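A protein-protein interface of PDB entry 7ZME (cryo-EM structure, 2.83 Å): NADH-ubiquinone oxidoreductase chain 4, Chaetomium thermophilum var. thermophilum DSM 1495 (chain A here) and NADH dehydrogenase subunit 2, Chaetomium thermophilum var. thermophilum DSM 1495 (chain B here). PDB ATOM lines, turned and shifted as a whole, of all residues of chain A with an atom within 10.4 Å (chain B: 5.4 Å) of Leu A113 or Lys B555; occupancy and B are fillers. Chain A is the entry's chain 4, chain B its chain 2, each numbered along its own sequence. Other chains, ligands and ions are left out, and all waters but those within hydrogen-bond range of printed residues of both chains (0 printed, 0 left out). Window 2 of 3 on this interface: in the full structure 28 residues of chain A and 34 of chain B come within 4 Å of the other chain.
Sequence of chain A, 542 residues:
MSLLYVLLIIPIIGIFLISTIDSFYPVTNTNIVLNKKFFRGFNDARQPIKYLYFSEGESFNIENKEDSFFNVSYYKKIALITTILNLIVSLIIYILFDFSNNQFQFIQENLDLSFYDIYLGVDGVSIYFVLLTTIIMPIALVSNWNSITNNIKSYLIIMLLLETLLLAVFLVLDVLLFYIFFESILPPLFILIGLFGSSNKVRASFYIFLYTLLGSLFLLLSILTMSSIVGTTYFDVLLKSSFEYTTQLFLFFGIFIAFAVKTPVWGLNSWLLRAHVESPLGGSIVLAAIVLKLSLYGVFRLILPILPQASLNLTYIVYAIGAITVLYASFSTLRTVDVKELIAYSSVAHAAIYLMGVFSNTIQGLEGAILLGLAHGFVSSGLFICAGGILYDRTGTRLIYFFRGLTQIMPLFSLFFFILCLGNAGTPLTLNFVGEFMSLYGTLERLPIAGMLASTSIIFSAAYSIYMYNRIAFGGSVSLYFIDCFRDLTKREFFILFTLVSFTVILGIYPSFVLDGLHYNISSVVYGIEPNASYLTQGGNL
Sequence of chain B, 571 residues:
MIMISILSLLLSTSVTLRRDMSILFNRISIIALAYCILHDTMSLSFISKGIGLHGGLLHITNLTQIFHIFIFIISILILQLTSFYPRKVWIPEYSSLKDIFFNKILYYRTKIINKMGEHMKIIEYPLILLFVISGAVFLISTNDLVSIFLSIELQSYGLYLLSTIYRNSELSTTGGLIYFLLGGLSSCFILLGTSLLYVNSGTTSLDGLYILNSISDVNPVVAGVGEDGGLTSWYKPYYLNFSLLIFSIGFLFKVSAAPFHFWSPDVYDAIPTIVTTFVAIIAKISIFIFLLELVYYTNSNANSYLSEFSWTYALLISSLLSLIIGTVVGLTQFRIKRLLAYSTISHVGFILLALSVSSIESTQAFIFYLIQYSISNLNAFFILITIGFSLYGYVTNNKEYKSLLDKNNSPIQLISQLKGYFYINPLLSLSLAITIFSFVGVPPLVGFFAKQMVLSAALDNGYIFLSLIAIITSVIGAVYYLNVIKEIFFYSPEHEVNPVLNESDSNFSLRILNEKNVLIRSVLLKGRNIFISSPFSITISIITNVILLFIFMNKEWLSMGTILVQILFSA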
ATOM      1  N   GLN A 108      23.101 -14.709  25.415  1.00  0.00           N
ATOM      2  CA  GLN A 108      23.260 -13.262  25.462  1.00  0.00           C
ATOM      3  C   GLN A 108      21.919 -12.613  25.753  1.00  0.00           C
ATOM      4  O   GLN A 108      20.914 -12.949  25.118  1.00  0.00           O
ATOM      5  CB  GLN A 108      23.831 -12.723  24.148  1.00  0.00           C
ATOM      6  CG  GLN A 108      23.898 -11.210  24.083  1.00  0.00           C
ATOM      7  CD  GLN A 108      24.988 -10.716  23.157  1.00  0.00           C
ATOM      8  OE1 GLN A 108      25.573 -11.488  22.399  1.00  0.00           O
ATOM      9  NE2 GLN A 108      25.268  -9.418  23.213  1.00  0.00           N
ATOM     10  N   GLU A 109      21.908 -11.682  26.706  1.00  0.00           N
ATOM     11  CA  GLU A 109      20.686 -10.965  27.044  1.00  0.00           C
ATOM     12  C   GLU A 109      20.190 -10.159  25.852  1.00  0.00           C
ATOM     13  O   GLU A 109      20.974  -9.531  25.135  1.00  0.00           O
ATOM     14  CB  GLU A 109      20.928 -10.040  28.237  1.00  0.00           C
ATOM     15  CG  GLU A 109      21.044 -10.756  29.569  1.00  0.00           C
ATOM     16  CD  GLU A 109      19.699 -11.162  30.129  1.00  0.00           C
ATOM     17  OE1 GLU A 109      18.705 -10.453  29.863  1.00  0.00           O
ATOM     18  OE2 GLU A 109      19.632 -12.188  30.838  1.00  0.00           O
ATOM     19  N   ASN A 110      18.875 -10.179  25.641  1.00  0.00           N
ATOM     20  CA  ASN A 110      18.265  -9.424  24.552  1.00  0.00           C
ATOM     21  C   ASN A 110      17.372  -8.304  25.069  1.00  0.00           C
ATOM     22  O   ASN A 110      17.611  -7.138  24.739  1.00  0.00           O
ATOM     23  CB  ASN A 110      17.473 -10.371  23.642  1.00  0.00           C
ATOM     24  CG  ASN A 110      17.278  -9.810  22.249  1.00  0.00           C
ATOM     25  OD1 ASN A 110      18.215  -9.295  21.638  1.00  0.00           O
ATOM     26  ND2 ASN A 110      16.057  -9.906  21.738  1.00  0.00           N
ATOM     27  N   LEU A 111      16.359  -8.623  25.880  1.00  0.00           N
ATOM     28  CA  LEU A 111      15.442  -7.628  26.447  1.00  0.00           C
ATOM     29  C   LEU A 111      14.844  -6.727  25.367  1.00  0.00           C
ATOM     30  O   LEU A 111      14.505  -5.569  25.619  1.00  0.00           O
ATOM     31  CB  LEU A 111      16.134  -6.792  27.525  1.00  0.00           C
ATOM     32  CG  LEU A 111      16.454  -7.527  28.828  1.00  0.00           C
ATOM     33  CD1 LEU A 111      16.824  -6.540  29.924  1.00  0.00           C
ATOM     34  CD2 LEU A 111      15.280  -8.396  29.257  1.00  0.00           C
ATOM     35  N   ASP A 112      14.709  -7.260  24.157  1.00  0.00           N
ATOM     36  CA  ASP A 112      14.181  -6.545  22.999  1.00  0.00           C
ATOM     37  C   ASP A 112      13.148  -7.406  22.289  1.00  0.00           C
ATOM     38  O   ASP A 112      13.189  -7.600  21.072  1.00  0.00           O
ATOM     39  CB  ASP A 112      15.302  -6.141  22.048  1.00  0.00           C
ATOM     40  N   LEU A 113      12.213  -7.950  23.067  1.00  0.00           N
ATOM     41  CA  LEU A 113      11.258  -8.940  22.586  1.00  0.00           C
ATOM     42  C   LEU A 113      10.481  -8.468  21.364  1.00  0.00           C
ATOM     43  O   LEU A 113       9.704  -7.511  21.440  1.00  0.00           O
ATOM     44  CB  LEU A 113      10.279  -9.312  23.702  1.00  0.00           C
ATOM     45  CG  LEU A 113      10.859 -10.063  24.902  1.00  0.00           C
ATOM     46  CD1 LEU A 113       9.745 -10.602  25.782  1.00  0.00           C
ATOM     47  CD2 LEU A 113      11.773 -11.184  24.443  1.00  0.00           C
ATOM     48  N   SER A 114      10.696  -9.132  20.236  1.00  0.00           N
ATOM     49  CA  SER A 114       9.870  -8.987  19.048  1.00  0.00           C
ATOM     50  C   SER A 114       9.059 -10.262  18.856  1.00  0.00           C
ATOM     51  O   SER A 114       9.081 -11.174  19.683  1.00  0.00           O
ATOM     52  CB  SER A 114      10.725  -8.679  17.817  1.00  0.00           C
ATOM     53  OG  SER A 114      11.684  -7.676  18.094  1.00  0.00           O
ATOM     54  N   PHE A 115       8.321 -10.311  17.753  1.00  0.00           N
ATOM     55  CA  PHE A 115       7.540 -11.501  17.444  1.00  0.00           C
ATOM     56  C   PHE A 115       8.449 -12.686  17.147  1.00  0.00           C
ATOM     57  O   PHE A 115       8.262 -13.781  17.688  1.00  0.00           O
ATOM     58  CB  PHE A 115       6.607 -11.201  16.274  1.00  0.00           C
ATOM     59  CG  PHE A 115       5.539 -10.203  16.609  1.00  0.00           C
ATOM     60  CD1 PHE A 115       4.395 -10.595  17.280  1.00  0.00           C
ATOM     61  CD2 PHE A 115       5.708  -8.863  16.318  1.00  0.00           C
ATOM     62  CE1 PHE A 115       3.417  -9.678  17.603  1.00  0.00           C
ATOM     63  CE2 PHE A 115       4.737  -7.944  16.644  1.00  0.00           C
ATOM     64  CZ  PHE A 115       3.588  -8.352  17.283  1.00  0.00           C
ATOM     65  N   TYR A 116       9.444 -12.481  16.292  1.00  0.00           N
ATOM     66  CA  TYR A 116      10.473 -13.473  16.023  1.00  0.00           C
ATOM     67  C   TYR A 116      11.809 -12.888  16.439  1.00  0.00           C
ATOM     68  O   TYR A 116      12.205 -11.828  15.947  1.00  0.00           O
ATOM     69  CB  TYR A 116      10.482 -13.868  14.546  1.00  0.00           C
ATOM     70  CG  TYR A 116       9.104 -14.144  14.005  1.00  0.00           C
ATOM     71  CD1 TYR A 116       8.494 -15.369  14.218  1.00  0.00           C
ATOM     72  CD2 TYR A 116       8.406 -13.177  13.300  1.00  0.00           C
ATOM     73  CE1 TYR A 116       7.235 -15.629  13.739  1.00  0.00           C
ATOM     74  CE2 TYR A 116       7.144 -13.428  12.813  1.00  0.00           C
ATOM     75  CZ  TYR A 116       6.561 -14.658  13.036  1.00  0.00           C
ATOM     76  OH  TYR A 116       5.300 -14.920  12.557  1.00  0.00           O
ATOM     77  N   ASP A 117      12.489 -13.567  17.353  1.00  0.00           N
ATOM     78  CA  ASP A 117      13.826 -13.185  17.777  1.00  0.00           C
ATOM     79  C   ASP A 117      14.711 -14.414  17.746  1.00  0.00           C
ATOM     80  O   ASP A 117      14.231 -15.543  17.851  1.00  0.00           O
ATOM     81  CB  ASP A 117      13.841 -12.578  19.178  1.00  0.00           C
ATOM     82  CG  ASP A 117      12.837 -11.467  19.340  1.00  0.00           C
ATOM     83  OD1 ASP A 117      13.148 -10.327  18.945  1.00  0.00           O
ATOM     84  OD2 ASP A 117      11.741 -11.735  19.867  1.00  0.00           O
ATOM     85  N   ILE A 118      16.009 -14.181  17.600  1.00  0.00           N
ATOM     86  CA  ILE A 118      16.993 -15.247  17.489  1.00  0.00           C
ATOM     87  C   ILE A 118      17.717 -15.348  18.823  1.00  0.00           C
ATOM     88  O   ILE A 118      18.432 -14.426  19.227  1.00  0.00           O
ATOM     89  CB  ILE A 118      17.965 -14.992  16.331  1.00  0.00           C
ATOM     90  CG1 ILE A 118      17.249 -15.194  14.997  1.00  0.00           C
ATOM     91  CG2 ILE A 118      19.175 -15.904  16.435  1.00  0.00           C
ATOM     92  CD1 ILE A 118      17.823 -14.381  13.874  1.00  0.00           C
ATOM     93  N   TYR A 119      17.524 -16.467  19.510  1.00  0.00           N
ATOM     94  CA  TYR A 119      18.183 -16.753  20.776  1.00  0.00           C
ATOM     95  C   TYR A 119      19.113 -17.936  20.570  1.00  0.00           C
ATOM     96  O   TYR A 119      18.688 -18.974  20.059  1.00  0.00           O
ATOM     97  CB  TYR A 119      17.164 -17.082  21.866  1.00  0.00           C
ATOM     98  CG  TYR A 119      15.958 -16.177  21.887  1.00  0.00           C
ATOM     99  CD1 TYR A 119      16.053 -14.869  22.332  1.00  0.00           C
ATOM    100  CD2 TYR A 119      14.718 -16.638  21.477  1.00  0.00           C
ATOM    101  CE1 TYR A 119      14.947 -14.044  22.358  1.00  0.00           C
ATOM    102  CE2 TYR A 119      13.611 -15.823  21.498  1.00  0.00           C
ATOM    103  CZ  TYR A 119      13.729 -14.528  21.942  1.00  0.00           C
ATOM    104  OH  TYR A 119      12.625 -13.710  21.965  1.00  0.00           O
ATOM    105  N   ASP A 174      14.858 -22.143  20.147  1.00  0.00           N
ATOM    106  CA  ASP A 174      13.437 -22.031  19.881  1.00  0.00           C
ATOM    107  C   ASP A 174      13.089 -22.999  18.761  1.00  0.00           C
ATOM    108  O   ASP A 174      13.889 -23.221  17.850  1.00  0.00           O
ATOM    109  CB  ASP A 174      13.076 -20.582  19.523  1.00  0.00           C
ATOM    110  CG  ASP A 174      11.605 -20.386  19.252  1.00  0.00           C
ATOM    111  OD1 ASP A 174      11.172 -20.640  18.111  1.00  0.00           O
ATOM    112  OD2 ASP A 174      10.878 -19.969  20.174  1.00  0.00           O
ATOM    113  N   GLY A 231       1.893 -21.122  23.705  1.00  0.00           N
ATOM    114  CA  GLY A 231       2.111 -19.701  23.568  1.00  0.00           C
ATOM    115  C   GLY A 231       3.497 -19.314  23.109  1.00  0.00           C
ATOM    116  O   GLY A 231       3.735 -18.130  22.846  1.00  0.00           O
ATOM    117  N   THR A 232       4.413 -20.270  23.003  1.00  0.00           N
ATOM    118  CA  THR A 232       5.768 -20.021  22.534  1.00  0.00           C
ATOM    119  C   THR A 232       6.404 -21.364  22.211  1.00  0.00           C
ATOM    120  O   THR A 232       5.835 -22.422  22.489  1.00  0.00           O
ATOM    121  CB  THR A 232       6.597 -19.248  23.568  1.00  0.00           C
ATOM    122  OG1 THR A 232       7.873 -18.913  23.011  1.00  0.00           O
ATOM    123  CG2 THR A 232       6.792 -20.063  24.820  1.00  0.00           C
ATOM    124  N   TYR A 234      10.063 -21.273  22.738  1.00  0.00           N
ATOM    125  CA  TYR A 234      11.329 -21.145  23.445  1.00  0.00           C
ATOM    126  C   TYR A 234      11.564 -22.385  24.295  1.00  0.00           C
ATOM    127  O   TYR A 234      10.653 -22.875  24.964  1.00  0.00           O
ATOM    128  CB  TYR A 234      11.318 -19.886  24.311  1.00  0.00           C
ATOM    129  CG  TYR A 234      12.618 -19.593  25.026  1.00  0.00           C
ATOM    130  CD1 TYR A 234      13.741 -19.178  24.326  1.00  0.00           C
ATOM    131  CD2 TYR A 234      12.711 -19.706  26.405  1.00  0.00           C
ATOM    132  CE1 TYR A 234      14.922 -18.902  24.978  1.00  0.00           C
ATOM    133  CE2 TYR A 234      13.886 -19.432  27.063  1.00  0.00           C
ATOM    134  CZ  TYR A 234      14.989 -19.032  26.347  1.00  0.00           C
ATOM    135  OH  TYR A 234      16.165 -18.758  27.005  1.00  0.00           O
ATOM    136  N   VAL A 237      10.586 -22.674  28.189  1.00  0.00           N
ATOM    137  CA  VAL A 237       9.147 -22.697  28.427  1.00  0.00           C
ATOM    138  C   VAL A 237       8.534 -23.981  27.882  1.00  0.00           C
ATOM    139  O   VAL A 237       7.739 -24.646  28.553  1.00  0.00           O
ATOM    140  CB  VAL A 237       8.485 -21.456  27.806  1.00  0.00           C
ATOM    141  CG1 VAL A 237       7.000 -21.436  28.118  1.00  0.00           C
ATOM    142  CG2 VAL A 237       9.177 -20.187  28.280  1.00  0.00           C
ATOM    143  N   MET B 553      13.425  -6.657  11.263  1.00  0.00           N
ATOM    144  CA  MET B 553      12.617  -5.415  11.220  1.00  0.00           C
ATOM    145  C   MET B 553      11.144  -5.754  11.453  1.00  0.00           C
ATOM    146  O   MET B 553      10.297  -4.894  11.167  1.00  0.00           O
ATOM    147  CB  MET B 553      12.746  -4.826   9.817  1.00  0.00           C
ATOM    148  CG  MET B 553      12.179  -5.746   8.755  1.00  0.00           C
ATOM    149  SD  MET B 553      12.149  -5.072   7.085  1.00  0.00           S
ATOM    150  CE  MET B 553      13.902  -4.901   6.761  1.00  0.00           C
ATOM    151  N   ASN B 554      10.834  -6.943  11.946  1.00  0.00           N
ATOM    152  CA  ASN B 554       9.427  -7.409  12.061  1.00  0.00           C
ATOM    153  C   ASN B 554       8.546  -6.674  13.071  1.00  0.00           C
ATOM    154  O   ASN B 554       7.331  -6.657  12.841  1.00  0.00           O
ATOM    155  CB  ASN B 554       9.373  -8.910  12.376  1.00  0.00           C
ATOM    156  CG  ASN B 554       9.969  -9.279  13.720  1.00  0.00           C
ATOM    157  OD1 ASN B 554       9.275  -9.283  14.734  1.00  0.00           O
ATOM    158  ND2 ASN B 554      11.247  -9.610  13.738  1.00  0.00           N
ATOM    159  N   LYS B 555       9.101  -6.095  14.139  1.00  0.00           N
ATOM    160  CA  LYS B 555       8.242  -5.622  15.259  1.00  0.00           C
ATOM    161  C   LYS B 555       7.200  -4.554  14.925  1.00  0.00           C
ATOM    162  O   LYS B 555       6.033  -4.854  15.132  1.00  0.00           O
ATOM    163  CB  LYS B 555       9.108  -5.203  16.450  1.00  0.00           C
ATOM    164  CG  LYS B 555       8.359  -5.012  17.760  1.00  0.00           C
ATOM    165  CD  LYS B 555       9.264  -4.722  18.929  1.00  0.00           C
ATOM    166  CE  LYS B 555       8.497  -4.446  20.203  1.00  0.00           C
ATOM    167  NZ  LYS B 555       7.497  -5.502  20.476  1.00  0.00           N
ATOM    168  N   GLU B 556       7.555  -3.426  14.324  1.00  0.00           N
ATOM    169  CA  GLU B 556       6.540  -2.352  14.135  1.00  0.00           C
ATOM    170  C   GLU B 556       5.480  -2.785  13.133  1.00  0.00           C
ATOM    171  O   GLU B 556       4.309  -2.480  13.360  1.00  0.00           O
ATOM    172  CB  GLU B 556       7.187  -1.019  13.762  1.00  0.00           C
ATOM    173  CG  GLU B 556       7.893  -0.341  14.921  1.00  0.00           C
ATOM    174  CD  GLU B 556       9.236  -0.941  15.294  1.00  0.00           C
ATOM    175  OE1 GLU B 556      10.211  -0.693  14.567  1.00  0.00           O
ATOM    176  OE2 GLU B 556       9.299  -1.660  16.303  1.00  0.00           O
ATOM    177  N   TRP B 557       5.894  -3.448  12.057  1.00  0.00           N
ATOM    178  CA  TRP B 557       4.972  -3.875  10.980  1.00  0.00           C
ATOM    179  C   TRP B 557       3.960  -4.884  11.515  1.00  0.00           C
ATOM    180  O   TRP B 557       2.777  -4.773  11.180  1.00  0.00           O
ATOM    181  CB  TRP B 557       5.812  -4.454   9.841  1.00  0.00           C
ATOM    182  CG  TRP B 557       5.073  -4.838   8.594  1.00  0.00           C
ATOM    183  CD1 TRP B 557       3.734  -4.750   8.351  1.00  0.00           C
ATOM    184  CD2 TRP B 557       5.658  -5.379   7.399  1.00  0.00           C
ATOM    185  NE1 TRP B 557       3.445  -5.206   7.095  1.00  0.00           N
ATOM    186  CE2 TRP B 557       4.608  -5.595   6.485  1.00  0.00           C
ATOM    187  CE3 TRP B 557       6.964  -5.697   7.013  1.00  0.00           C
ATOM    188  CZ2 TRP B 557       4.824  -6.118   5.212  1.00  0.00           C
ATOM    189  CZ3 TRP B 557       7.178  -6.215   5.756  1.00  0.00           C
ATOM    190  CH2 TRP B 557       6.121  -6.420   4.869  1.00  0.00           C
ATOM    191  N   LEU B 558       4.411  -5.829  12.324  1.00  0.00           N
ATOM    192  CA  LEU B 558       3.495  -6.873  12.817  1.00  0.00           C
ATOM    193  C   LEU B 558       2.645  -6.271  13.929  1.00  0.00           C
ATOM    194  O   LEU B 558       1.502  -6.707  14.086  1.00  0.00           O
ATOM    195  CB  LEU B 558       4.310  -8.086  13.279  1.00  0.00           C
ATOM    196  CG  LEU B 558       4.779  -9.019  12.168  1.00  0.00           C
ATOM    197  CD1 LEU B 558       5.641 -10.131  12.731  1.00  0.00           C
ATOM    198  CD2 LEU B 558       3.593  -9.595  11.418  1.00  0.00           C
ATOM    199  N   SER B 559       3.197  -5.293  14.655  1.00  0.00           N
ATOM    200  CA  SER B 559       2.437  -4.707  15.751  1.00  0.00           C
ATOM    201  C   SER B 559       1.352  -3.769  15.244  1.00  0.00           C
ATOM    202  O   SER B 559       0.353  -3.551  15.935  1.00  0.00           O
ATOM    203  CB  SER B 559       3.372  -3.972  16.702  1.00  0.00           C
ATOM    204  OG  SER B 559       4.527  -4.745  16.969  1.00  0.00           O
ATOM    205  N   MET B 560       1.532  -3.205  14.048  1.00  0.00           N
ATOM    206  CA  MET B 560       0.471  -2.408  13.447  1.00  0.00           C
ATOM    207  C   MET B 560      -0.783  -3.243  13.233  1.00  0.00           C
ATOM    208  O   MET B 560      -1.896  -2.797  13.533  1.00  0.00           O
ATOM    209  CB  MET B 560       0.938  -1.823  12.119  1.00  0.00           C
ATOM    210  CG  MET B 560      -0.101  -0.933  11.459  1.00  0.00           C
ATOM    211  SD  MET B 560       0.470  -0.239   9.904  1.00  0.00           S
ATOM    212  CE  MET B 560       0.430  -1.707   8.882  1.00  0.00           C
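The side-chain amide oxygen (OD1) of Asn B554 sits at hydrogen-bond distance from the backbone NH (N) of Phe A115 (3.3 Å). O of Tyr A116 lies within hydrogen-bond range of ND2 of Asn B554, 3.3 Å away. NZ of Lys B555 is in hydrogen-bond range of O of Leu A113 (3.1 Å).
The backbone carbonyl oxygen (O) of Asp A112 sits at hydrogen-bond distance from the side-chain hydroxyl (OG) of Ser A114 (3.3 Å). The backbone NH (N) of Ser A114 lies within hydrogen-bond range of the side-chain carboxylate (OD2) of Asp A117, 2.8 Å away.
Among the printed residues, pairs that only touch across the chains: Phe A115 with Ser B559 (3.2 Å), Phe A115 with Leu B558 (3.4 Å), Ser A114 with Asn B554 (3.5 Å), Tyr A116 with Leu B558 (3.6 Å), Phe A115 with Lys B555 (3.7 Å) and Ser A114 with Lys B555 (3.9 Å).
Leu A113 touches just one residue of chain B: Lys B555. Lys B555 touches three residues of chain A. Of chain A, only Ser A114, Phe A115 and Tyr A116 come within 4 Å of Asn B554. Glu B556 touches none of the printed residues of chain A. Printed residues of chain A within 4 Å of Ser B559: Phe A115 (3.2 Å). Printed residues of chain A within 4 Å of Leu B558: Phe A115 (3.4 Å) and Tyr A116 (3.6 Å). Printed residues of chain B within 4 Å of Ser A114: Asn B554 and Lys B555. Trp B557 touches none of the printed residues of chain A. Glu A109 touches none of the printed residues of chain B. The nearest printed residue of chain B that does not touch Leu A113 is Asn B554 (6.8 Å). The nearest printed residue of chain B that does not touch Ser A114 is Glu B556 (6.7 Å).
Hydrophobic or aromatic side chains of chain A within 4 Å of the printed part of chain B: Phe A115 and Tyr A116. Printed residues of chain B that touch a printed residue of chain A: Asn B554, Lys B555, Leu B558 and Ser B559. Hydrophobic or aromatic side chains of chain B within 4 Å of the printed part of chain A: Leu B558. Among the printed residues, 9 pairs touch across the chains. Among the printed residues, no Asp or Glu carboxylate lies within 4 Å of a Lys or Arg side-chain nitrogen of the other chain.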
